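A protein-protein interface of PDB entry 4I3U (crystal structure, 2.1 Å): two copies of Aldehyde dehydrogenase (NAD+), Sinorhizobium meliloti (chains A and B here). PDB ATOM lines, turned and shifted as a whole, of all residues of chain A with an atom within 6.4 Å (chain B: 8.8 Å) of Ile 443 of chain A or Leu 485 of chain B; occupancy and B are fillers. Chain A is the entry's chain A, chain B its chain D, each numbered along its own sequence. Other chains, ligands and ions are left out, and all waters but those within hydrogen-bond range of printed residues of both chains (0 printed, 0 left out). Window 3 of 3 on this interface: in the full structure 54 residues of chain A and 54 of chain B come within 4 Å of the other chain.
Hydrophobic or aromatic side chains of chain A that line the printed part of chain B: Ile 433 and Ile 443.
Along chain A the printed residues that touch a printed residue of chain B span positions 433 to 445.
Of the 15 printed residues of chain B, 7 touch a printed residue of chain A.
Hydrophobic or aromatic side chains of chain B within 4 Å of the printed part of chain A: Phe 483, Leu 485 and Pro 486.
No position is printed for both chains.
Of the 12 pairs that touch across the chains among the printed residues, none has its exchanged pair printed and touching as well.
Ser 419 of chain A touches none of the printed residues of chain B.
No residue of chain B comes within 4 Å of Val 421 of chain A.
Printed residues of chain B within 4 Å of Asn 442 of chain A: Ser 484 (2.7 Å).
Of chain B, only Arg 142, Ser 484, Leu 485 and Pro 486 come within 4 Å of Ile 443 of chain A.
Printed residues of chain A within 4 Å of Lys 140 of chain B: Glu 445 (3.2 Å).
Of chain A, only Ile 443 (3.8 Å) comes within 4 Å of Leu 485 of chain B.
Of the printed residues of chain A, Pro 486 of chain B touches Ile 443.
The nearest residue of chain A that does not touch Leu 485 of chain B is Met 429 of chain A (4.4 Å).
The backbone carbonyl oxygen (O) of Ser 419 of chain A sits at hydrogen-bond distance from the backbone NH (N) of Asn 442 of chain A.
NH1 of Arg 142 of chain B is in hydrogen-bond range of OG of Ser 484 of chain B (2.9 Å).
O of Val 421 of chain A lies within hydrogen-bond range of N of Trp 444 of chain A.
The backbone carbonyl oxygen of Cys 133 of chain B sits at hydrogen-bond distance from the backbone NH of Lys 140 of chain B.
The backbone NH of Val 421 of chain A sits at hydrogen-bond distance from the backbone carbonyl oxygen of Asn 442 of chain A (2.8 Å).
N of Cys 133 of chain B lies within hydrogen-bond range of O of Arg 142 of chain B (3.0 Å).
The guanidinium group (NH2) of Arg 142 of chain B lies within hydrogen-bond range of the backbone carbonyl oxygen (O) of Trp 444 of chain A (3.3 Å).
O of Ser 484 of chain B sits at hydrogen-bond distance from N of Ile 443 of chain A, at 3.0 Å.
The side-chain hydroxyl (OG) of Ser 484 of chain B is in hydrogen-bond range of the side-chain amide oxygen (OD1) of Asn 442 of chain A, at 2.7 Å.
O of Thr 482 of chain B sits at hydrogen-bond distance from N of Val 441 of chain A, 2.9 Å away.
The guanidinium group (NH1) of Arg 142 of chain B sits at hydrogen-bond distance from the backbone carbonyl oxygen (O) of Ile 443 of chain A (2.9 Å).
O of Val 441 of chain A sits at hydrogen-bond distance from N of Ser 484 of chain B (3.2 Å).
Among the printed residues, merely in contact across the chains: Val 441 of chain A with Phe 483 of chain B (3.0 Å), Glu 445 of chain A with Lys 140 of chain B (3.2 Å), Glu 445 of chain A with Arg 142 of chain B (3.6 Å), Ile 433 of chain A with Phe 483 of chain B (3.7 Å), Ile 443 of chain A with Leu 485 of chain B (3.8 Å) and Ile 443 of chain A with Pro 486 of chain B (3.8 Å).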
ATOM      1  N   SER A 419     -14.195 -27.676   9.117  1.00  0.00           N
ATOM      2  CA  SER A 419     -13.424 -28.304   8.063  1.00  0.00           C
ATOM      3  C   SER A 419     -11.947 -28.117   8.316  1.00  0.00           C
ATOM      4  O   SER A 419     -11.551 -27.180   9.006  1.00  0.00           O
ATOM      5  CB  SER A 419     -13.771 -27.683   6.711  1.00  0.00           C
ATOM      6  OG  SER A 419     -13.473 -26.286   6.709  1.00  0.00           O
ATOM      7  N   GLY A 420     -11.143 -29.015   7.761  1.00  0.00           N
ATOM      8  CA  GLY A 420      -9.695 -28.872   7.780  1.00  0.00           C
ATOM      9  C   GLY A 420      -9.172 -28.955   6.344  1.00  0.00           C
ATOM     10  O   GLY A 420      -9.688 -29.706   5.516  1.00  0.00           O
ATOM     11  N   VAL A 421      -8.141 -28.179   6.050  1.00  0.00           N
ATOM     12  CA  VAL A 421      -7.532 -28.232   4.735  1.00  0.00           C
ATOM     13  C   VAL A 421      -6.014 -28.294   4.866  1.00  0.00           C
ATOM     14  O   VAL A 421      -5.412 -27.434   5.491  1.00  0.00           O
ATOM     15  CB  VAL A 421      -7.928 -27.022   3.857  1.00  0.00           C
ATOM     16  CG1 VAL A 421      -7.302 -27.165   2.458  1.00  0.00           C
ATOM     17  CG2 VAL A 421      -9.422 -26.928   3.745  1.00  0.00           C
ATOM     18  N   CYS A 422      -5.409 -29.311   4.268  1.00  0.00           N
ATOM     19  CA  CYS A 422      -3.952 -29.458   4.296  1.00  0.00           C
ATOM     20  C   CYS A 422      -3.368 -29.106   2.931  1.00  0.00           C
ATOM     21  O   CYS A 422      -3.614 -29.805   1.947  1.00  0.00           O
ATOM     22  CB  CYS A 422      -3.577 -30.881   4.677  1.00  0.00           C
ATOM     23  SG  CYS A 422      -4.225 -31.343   6.317  1.00  0.00           S
ATOM     24  N   THR A 423      -2.634 -28.008   2.874  1.00  0.00           N
ATOM     25  CA  THR A 423      -2.036 -27.530   1.619  1.00  0.00           C
ATOM     26  C   THR A 423      -1.025 -26.479   2.007  1.00  0.00           C
ATOM     27  O   THR A 423      -1.062 -25.992   3.127  1.00  0.00           O
ATOM     28  CB  THR A 423      -3.082 -26.902   0.710  1.00  0.00           C
ATOM     29  OG1 THR A 423      -2.503 -26.570  -0.567  1.00  0.00           O
ATOM     30  CG2 THR A 423      -3.685 -25.672   1.372  1.00  0.00           C
ATOM     31  N   TYR A 426      -0.998 -20.986  -0.861  1.00  0.00           N
ATOM     32  CA  TYR A 426      -1.863 -19.957  -0.280  1.00  0.00           C
ATOM     33  C   TYR A 426      -3.097 -19.683  -1.139  1.00  0.00           C
ATOM     34  O   TYR A 426      -4.188 -19.493  -0.641  1.00  0.00           O
ATOM     35  CB  TYR A 426      -1.134 -18.611  -0.080  1.00  0.00           C
ATOM     36  CG  TYR A 426      -2.143 -17.544   0.284  1.00  0.00           C
ATOM     37  CD1 TYR A 426      -2.395 -17.174   1.432  1.00  0.00           C
ATOM     38  CD2 TYR A 426      -2.887 -17.017  -0.517  1.00  0.00           C
ATOM     39  CE1 TYR A 426      -3.376 -16.231   1.726  1.00  0.00           C
ATOM     40  CE2 TYR A 426      -3.860 -16.113  -0.178  1.00  0.00           C
ATOM     41  CZ  TYR A 426      -4.106 -15.715   0.930  1.00  0.00           C
ATOM     42  OH  TYR A 426      -5.089 -14.789   1.243  1.00  0.00           O
ATOM     43  N   MET A 429      -5.493 -22.364  -0.512  1.00  0.00           N
ATOM     44  CA  MET A 429      -5.972 -22.108   0.858  1.00  0.00           C
ATOM     45  C   MET A 429      -7.116 -21.107   0.868  1.00  0.00           C
ATOM     46  O   MET A 429      -8.173 -21.347   1.467  1.00  0.00           O
ATOM     47  CB  MET A 429      -4.863 -21.477   1.659  1.00  0.00           C
ATOM     48  CG  MET A 429      -4.423 -22.227   2.841  1.00  0.00           C
ATOM     49  SD  MET A 429      -3.025 -21.381   3.579  1.00  0.00           S
ATOM     50  CE  MET A 429      -1.828 -22.757   3.539  1.00  0.00           C
ATOM     51  N   GLN A 430      -6.888 -19.947   0.255  1.00  0.00           N
ATOM     52  CA  GLN A 430      -7.885 -18.895   0.389  1.00  0.00           C
ATOM     53  C   GLN A 430      -9.137 -19.224  -0.406  1.00  0.00           C
ATOM     54  O   GLN A 430     -10.233 -18.850   0.007  1.00  0.00           O
ATOM     55  CB  GLN A 430      -7.303 -17.468   0.235  1.00  0.00           C
ATOM     56  CG  GLN A 430      -7.592 -16.578  -0.922  1.00  0.00           C
ATOM     57  CD  GLN A 430      -9.030 -16.332  -1.266  1.00  0.00           C
ATOM     58  OE1 GLN A 430      -9.866 -16.031  -0.442  1.00  0.00           O
ATOM     59  NE2 GLN A 430      -9.312 -16.442  -2.513  1.00  0.00           N
ATOM     60  N   TYR A 432     -10.394 -22.292  -0.746  1.00  0.00           N
ATOM     61  CA  TYR A 432     -11.158 -23.142   0.179  1.00  0.00           C
ATOM     62  C   TYR A 432     -11.773 -22.384   1.355  1.00  0.00           C
ATOM     63  O   TYR A 432     -12.937 -22.615   1.694  1.00  0.00           O
ATOM     64  CB  TYR A 432     -10.307 -24.304   0.696  1.00  0.00           C
ATOM     65  CG  TYR A 432     -10.201 -25.407  -0.327  1.00  0.00           C
ATOM     66  CD1 TYR A 432      -9.263 -25.337  -1.353  1.00  0.00           C
ATOM     67  CD2 TYR A 432     -11.053 -26.493  -0.280  1.00  0.00           C
ATOM     68  CE1 TYR A 432      -9.165 -26.341  -2.293  1.00  0.00           C
ATOM     69  CE2 TYR A 432     -10.955 -27.506  -1.197  1.00  0.00           C
ATOM     70  CZ  TYR A 432     -10.017 -27.423  -2.215  1.00  0.00           C
ATOM     71  OH  TYR A 432      -9.953 -28.433  -3.143  1.00  0.00           O
ATOM     72  N   ILE A 433     -11.000 -21.496   1.969  1.00  0.00           N
ATOM     73  CA  ILE A 433     -11.540 -20.645   3.032  1.00  0.00           C
ATOM     74  C   ILE A 433     -12.801 -19.906   2.574  1.00  0.00           C
ATOM     75  O   ILE A 433     -13.800 -19.887   3.283  1.00  0.00           O
ATOM     76  CB  ILE A 433     -10.487 -19.659   3.606  1.00  0.00           C
ATOM     77  CG1 ILE A 433      -9.454 -20.411   4.433  1.00  0.00           C
ATOM     78  CG2 ILE A 433     -11.157 -18.610   4.508  1.00  0.00           C
ATOM     79  CD1 ILE A 433      -8.168 -19.604   4.745  1.00  0.00           C
ATOM     80  N   VAL A 441     -13.023 -22.944   8.872  1.00  0.00           N
ATOM     81  CA  VAL A 441     -12.053 -23.611   8.014  1.00  0.00           C
ATOM     82  C   VAL A 441     -10.685 -23.576   8.702  1.00  0.00           C
ATOM     83  O   VAL A 441     -10.082 -22.515   8.885  1.00  0.00           O
ATOM     84  CB  VAL A 441     -11.947 -22.947   6.649  1.00  0.00           C
ATOM     85  CG1 VAL A 441     -10.901 -23.659   5.789  1.00  0.00           C
ATOM     86  CG2 VAL A 441     -13.285 -22.952   5.957  1.00  0.00           C
ATOM     87  N   ASN A 442     -10.205 -24.746   9.103  1.00  0.00           N
ATOM     88  CA  ASN A 442      -8.887 -24.830   9.712  1.00  0.00           C
ATOM     89  C   ASN A 442      -7.814 -25.246   8.707  1.00  0.00           C
ATOM     90  O   ASN A 442      -7.882 -26.339   8.103  1.00  0.00           O
ATOM     91  CB  ASN A 442      -8.905 -25.788  10.905  1.00  0.00           C
ATOM     92  CG  ASN A 442      -9.686 -25.229  12.094  1.00  0.00           C
ATOM     93  OD1 ASN A 442      -9.647 -24.026  12.373  1.00  0.00           O
ATOM     94  ND2 ASN A 442     -10.359 -26.103  12.824  1.00  0.00           N
ATOM     95  N   ILE A 443      -6.821 -24.384   8.502  1.00  0.00           N
ATOM     96  CA  ILE A 443      -5.692 -24.755   7.633  1.00  0.00           C
ATOM     97  C   ILE A 443      -4.687 -25.542   8.444  1.00  0.00           C
ATOM     98  O   ILE A 443      -4.184 -25.067   9.456  1.00  0.00           O
ATOM     99  CB  ILE A 443      -5.045 -23.519   6.967  1.00  0.00           C
ATOM    100  CG1 ILE A 443      -6.105 -22.743   6.173  1.00  0.00           C
ATOM    101  CG2 ILE A 443      -3.892 -23.912   6.075  1.00  0.00           C
ATOM    102  CD1 ILE A 443      -6.942 -23.625   5.276  1.00  0.00           C
ATOM    103  N   TRP A 444      -4.428 -26.775   8.013  1.00  0.00           N
ATOM    104  CA  TRP A 444      -3.462 -27.644   8.680  1.00  0.00           C
ATOM    105  C   TRP A 444      -3.832 -27.989  10.123  1.00  0.00           C
ATOM    106  O   TRP A 444      -2.963 -28.129  10.994  1.00  0.00           O
ATOM    107  CB  TRP A 444      -2.043 -27.051   8.618  1.00  0.00           C
ATOM    108  CG  TRP A 444      -1.303 -27.509   7.409  1.00  0.00           C
ATOM    109  CD1 TRP A 444      -0.874 -26.745   6.354  1.00  0.00           C
ATOM    110  CD2 TRP A 444      -0.915 -28.856   7.109  1.00  0.00           C
ATOM    111  NE1 TRP A 444      -0.241 -27.533   5.440  1.00  0.00           N
ATOM    112  CE2 TRP A 444      -0.249 -28.834   5.872  1.00  0.00           C
ATOM    113  CE3 TRP A 444      -1.068 -30.072   7.769  1.00  0.00           C
ATOM    114  CZ2 TRP A 444       0.276 -29.982   5.275  1.00  0.00           C
ATOM    115  CZ3 TRP A 444      -0.555 -31.232   7.173  1.00  0.00           C
ATOM    116  CH2 TRP A 444       0.112 -31.173   5.940  1.00  0.00           C
ATOM    117  N   GLU A 445      -5.124 -28.142  10.373  1.00  0.00           N
ATOM    118  CA  GLU A 445      -5.572 -28.655  11.648  1.00  0.00           C
ATOM    119  C   GLU A 445      -6.829 -29.464  11.383  1.00  0.00           C
ATOM    120  O   GLU A 445      -7.435 -29.346  10.311  1.00  0.00           O
ATOM    121  CB  GLU A 445      -5.824 -27.510  12.631  1.00  0.00           C
ATOM    122  CG  GLU A 445      -4.797 -27.420  13.777  1.00  0.00           C
ATOM    123  CD  GLU A 445      -4.739 -28.689  14.670  1.00  0.00           C
ATOM    124  OE1 GLU A 445      -5.648 -29.556  14.590  1.00  0.00           O
ATOM    125  OE2 GLU A 445      -3.768 -28.812  15.460  1.00  0.00           O
ATOM    126  N   PHE B 131      -7.853 -13.878  16.911  1.00  0.00           N
ATOM    127  CA  PHE B 131      -7.512 -14.504  18.189  1.00  0.00           C
ATOM    128  C   PHE B 131      -6.145 -15.175  18.099  1.00  0.00           C
ATOM    129  O   PHE B 131      -5.839 -15.858  17.110  1.00  0.00           O
ATOM    130  CB  PHE B 131      -8.536 -15.571  18.536  1.00  0.00           C
ATOM    131  CG  PHE B 131      -9.930 -15.041  18.741  1.00  0.00           C
ATOM    132  CD1 PHE B 131     -10.407 -14.807  20.020  1.00  0.00           C
ATOM    133  CD2 PHE B 131     -10.770 -14.789  17.661  1.00  0.00           C
ATOM    134  CE1 PHE B 131     -11.688 -14.309  20.230  1.00  0.00           C
ATOM    135  CE2 PHE B 131     -12.064 -14.282  17.861  1.00  0.00           C
ATOM    136  CZ  PHE B 131     -12.530 -14.042  19.139  1.00  0.00           C
ATOM    137  N   SER B 132      -5.346 -15.026  19.147  1.00  0.00           N
ATOM    138  CA  SER B 132      -4.109 -15.785  19.290  1.00  0.00           C
ATOM    139  C   SER B 132      -4.481 -17.046  20.032  1.00  0.00           C
ATOM    140  O   SER B 132      -5.396 -17.034  20.868  1.00  0.00           O
ATOM    141  CB  SER B 132      -3.076 -14.989  20.084  1.00  0.00           C
ATOM    142  OG  SER B 132      -2.545 -13.934  19.303  1.00  0.00           O
ATOM    143  N   CYS B 133      -3.806 -18.141  19.722  1.00  0.00           N
ATOM    144  CA  CYS B 133      -4.225 -19.423  20.236  1.00  0.00           C
ATOM    145  C   CYS B 133      -3.311 -20.054  21.304  1.00  0.00           C
ATOM    146  O   CYS B 133      -3.587 -21.175  21.702  1.00  0.00           O
ATOM    147  CB  CYS B 133      -4.423 -20.430  19.091  1.00  0.00           C
ATOM    148  SG  CYS B 133      -5.749 -20.048  17.913  1.00  0.00           S
ATOM    149  N   LYS B 140      -1.887 -23.407  20.967  1.00  0.00           N
ATOM    150  CA  LYS B 140      -1.068 -23.696  19.793  1.00  0.00           C
ATOM    151  C   LYS B 140      -0.561 -22.442  19.120  1.00  0.00           C
ATOM    152  O   LYS B 140      -1.171 -21.393  19.254  1.00  0.00           O
ATOM    153  CB  LYS B 140      -1.881 -24.498  18.827  1.00  0.00           C
ATOM    154  CG  LYS B 140      -1.926 -25.976  19.176  1.00  0.00           C
ATOM    155  CD  LYS B 140      -3.072 -26.607  18.464  1.00  0.00           C
ATOM    156  CE  LYS B 140      -3.034 -28.145  18.471  1.00  0.00           C
ATOM    157  NZ  LYS B 140      -2.109 -28.713  19.483  1.00  0.00           N
ATOM    158  N   ALA B 141       0.550 -22.563  18.400  1.00  0.00           N
ATOM    159  CA  ALA B 141       1.134 -21.428  17.704  1.00  0.00           C
ATOM    160  C   ALA B 141       0.292 -21.195  16.444  1.00  0.00           C
ATOM    161  O   ALA B 141       0.626 -21.641  15.350  1.00  0.00           O
ATOM    162  CB  ALA B 141       2.600 -21.703  17.379  1.00  0.00           C
ATOM    163  N   ARG B 142      -0.808 -20.475  16.621  1.00  0.00           N
ATOM    164  CA  ARG B 142      -1.815 -20.358  15.603  1.00  0.00           C
ATOM    165  C   ARG B 142      -2.665 -19.127  15.829  1.00  0.00           C
ATOM    166  O   ARG B 142      -2.831 -18.672  16.972  1.00  0.00           O
ATOM    167  CB  ARG B 142      -2.671 -21.613  15.685  1.00  0.00           C
ATOM    168  CG  ARG B 142      -3.856 -21.657  14.773  1.00  0.00           C
ATOM    169  CD  ARG B 142      -4.464 -23.090  14.735  1.00  0.00           C
ATOM    170  NE  ARG B 142      -3.563 -24.007  14.048  1.00  0.00           N
ATOM    171  CZ  ARG B 142      -3.599 -24.217  12.730  1.00  0.00           C
ATOM    172  NH1 ARG B 142      -4.549 -23.634  11.989  1.00  0.00           N
ATOM    173  NH2 ARG B 142      -2.717 -25.022  12.142  1.00  0.00           N
ATOM    174  N   LYS B 143      -3.223 -18.601  14.737  1.00  0.00           N
ATOM    175  CA  LYS B 143      -4.157 -17.479  14.816  1.00  0.00           C
ATOM    176  C   LYS B 143      -5.484 -17.874  14.231  1.00  0.00           C
ATOM    177  O   LYS B 143      -5.547 -18.595  13.223  1.00  0.00           O
ATOM    178  CB  LYS B 143      -3.622 -16.209  14.134  1.00  0.00           C
ATOM    179  CG  LYS B 143      -2.525 -15.488  14.927  1.00  0.00           C
ATOM    180  CD  LYS B 143      -1.927 -14.328  14.119  1.00  0.00           C
ATOM    181  CE  LYS B 143      -0.832 -13.621  14.909  1.00  0.00           C
ATOM    182  NZ  LYS B 143      -1.395 -12.631  15.867  1.00  0.00           N
ATOM    183  N   ILE B 144      -6.550 -17.403  14.870  1.00  0.00           N
ATOM    184  CA  ILE B 144      -7.896 -17.506  14.316  1.00  0.00           C
ATOM    185  C   ILE B 144      -8.345 -16.133  13.812  1.00  0.00           C
ATOM    186  O   ILE B 144      -8.143 -15.120  14.484  1.00  0.00           O
ATOM    187  CB  ILE B 144      -8.872 -18.029  15.389  1.00  0.00           C
ATOM    188  CG1 ILE B 144      -8.573 -19.499  15.699  1.00  0.00           C
ATOM    189  CG2 ILE B 144     -10.344 -17.941  14.942  1.00  0.00           C
ATOM    190  CD1 ILE B 144      -9.253 -20.003  16.956  1.00  0.00           C
ATOM    191  N   PHE B 145      -8.943 -16.110  12.628  1.00  0.00           N
ATOM    192  CA  PHE B 145      -9.398 -14.869  11.985  1.00  0.00           C
ATOM    193  C   PHE B 145     -10.905 -14.977  11.747  1.00  0.00           C
ATOM    194  O   PHE B 145     -11.428 -16.067  11.544  1.00  0.00           O
ATOM    195  CB  PHE B 145      -8.684 -14.636  10.639  1.00  0.00           C
ATOM    196  CG  PHE B 145      -7.182 -14.599  10.745  1.00  0.00           C
ATOM    197  CD1 PHE B 145      -6.445 -15.782  10.743  1.00  0.00           C
ATOM    198  CD2 PHE B 145      -6.509 -13.385  10.874  1.00  0.00           C
ATOM    199  CE1 PHE B 145      -5.087 -15.741  10.861  1.00  0.00           C
ATOM    200  CE2 PHE B 145      -5.140 -13.351  11.002  1.00  0.00           C
ATOM    201  CZ  PHE B 145      -4.428 -14.518  10.992  1.00  0.00           C
ATOM    202  N   THR B 482     -14.964 -18.490  10.675  1.00  0.00           N
ATOM    203  CA  THR B 482     -13.613 -18.347  11.204  1.00  0.00           C
ATOM    204  C   THR B 482     -12.660 -19.178  10.380  1.00  0.00           C
ATOM    205  O   THR B 482     -13.045 -20.203   9.809  1.00  0.00           O
ATOM    206  CB  THR B 482     -13.498 -18.834  12.658  1.00  0.00           C
ATOM    207  OG1 THR B 482     -13.641 -20.263  12.684  1.00  0.00           O
ATOM    208  CG2 THR B 482     -14.563 -18.188  13.542  1.00  0.00           C
ATOM    209  N   PHE B 483     -11.410 -18.749  10.324  1.00  0.00           N
ATOM    210  CA  PHE B 483     -10.390 -19.622   9.764  1.00  0.00           C
ATOM    211  C   PHE B 483      -9.150 -19.449  10.601  1.00  0.00           C
ATOM    212  O   PHE B 483      -8.956 -18.395  11.195  1.00  0.00           O
ATOM    213  CB  PHE B 483     -10.139 -19.333   8.269  1.00  0.00           C
ATOM    214  CG  PHE B 483      -9.662 -17.926   7.975  1.00  0.00           C
ATOM    215  CD1 PHE B 483     -10.577 -16.911   7.759  1.00  0.00           C
ATOM    216  CD2 PHE B 483      -8.300 -17.641   7.873  1.00  0.00           C
ATOM    217  CE1 PHE B 483     -10.162 -15.607   7.455  1.00  0.00           C
ATOM    218  CE2 PHE B 483      -7.875 -16.343   7.567  1.00  0.00           C
ATOM    219  CZ  PHE B 483      -8.818 -15.338   7.367  1.00  0.00           C
ATOM    220  N   SER B 484      -8.343 -20.495  10.674  1.00  0.00           N
ATOM    221  CA  SER B 484      -7.122 -20.442  11.454  1.00  0.00           C
ATOM    222  C   SER B 484      -5.940 -20.846  10.589  1.00  0.00           C
ATOM    223  O   SER B 484      -6.072 -21.712   9.713  1.00  0.00           O
ATOM    224  CB  SER B 484      -7.230 -21.296  12.720  1.00  0.00           C
ATOM    225  OG  SER B 484      -7.275 -22.674  12.411  1.00  0.00           O
ATOM    226  N   LEU B 485      -4.812 -20.177  10.820  1.00  0.00           N
ATOM    227  CA  LEU B 485      -3.561 -20.429  10.119  1.00  0.00           C
ATOM    228  C   LEU B 485      -2.470 -20.769  11.116  1.00  0.00           C
ATOM    229  O   LEU B 485      -2.446 -20.213  12.229  1.00  0.00           O
ATOM    230  CB  LEU B 485      -3.135 -19.154   9.361  1.00  0.00           C
ATOM    231  CG  LEU B 485      -4.171 -18.557   8.391  1.00  0.00           C
ATOM    232  CD1 LEU B 485      -3.652 -17.253   7.782  1.00  0.00           C
ATOM    233  CD2 LEU B 485      -4.443 -19.561   7.310  1.00  0.00           C
ATOM    234  N   PRO B 486      -1.548 -21.668  10.720  1.00  0.00           N
ATOM    235  CA  PRO B 486      -0.339 -21.892  11.523  1.00  0.00           C
ATOM    236  C   PRO B 486       0.378 -20.563  11.715  1.00  0.00           C
ATOM    237  O   PRO B 486       0.397 -19.765  10.798  1.00  0.00           O
ATOM    238  CB  PRO B 486       0.516 -22.814  10.634  1.00  0.00           C
ATOM    239  CG  PRO B 486      -0.463 -23.441   9.688  1.00  0.00           C
ATOM    240  CD  PRO B 486      -1.516 -22.407   9.438  1.00  0.00           C
ATOM    241  N   TRP B 487       0.906 -20.301  12.902  1.00  0.00           N
ATOM    242  CA  TRP B 487       1.625 -19.061  13.116  1.00  0.00           C
ATOM    243  C   TRP B 487       2.828 -19.297  14.040  1.00  0.00           C
ATOM    244  O   TRP B 487       2.780 -18.946  15.220  1.00  0.00           O
ATOM    245  CB  TRP B 487       0.661 -17.980  13.656  1.00  0.00           C
ATOM    246  CG  TRP B 487       1.140 -16.618  13.295  1.00  0.00           C
ATOM    247  CD1 TRP B 487       2.015 -15.858  13.992  1.00  0.00           C
ATOM    248  CD2 TRP B 487       0.808 -15.871  12.123  1.00  0.00           C
ATOM    249  NE1 TRP B 487       2.268 -14.702  13.326  1.00  0.00           N
ATOM    250  CE2 TRP B 487       1.538 -14.686  12.169  1.00  0.00           C
ATOM    251  CE3 TRP B 487      -0.053 -16.075  11.042  1.00  0.00           C
ATOM    252  CZ2 TRP B 487       1.455 -13.710  11.186  1.00  0.00           C
ATOM    253  CZ3 TRP B 487      -0.128 -15.066  10.043  1.00  0.00           C
ATOM    254  CH2 TRP B 487       0.616 -13.910  10.141  1.00  0.00           C
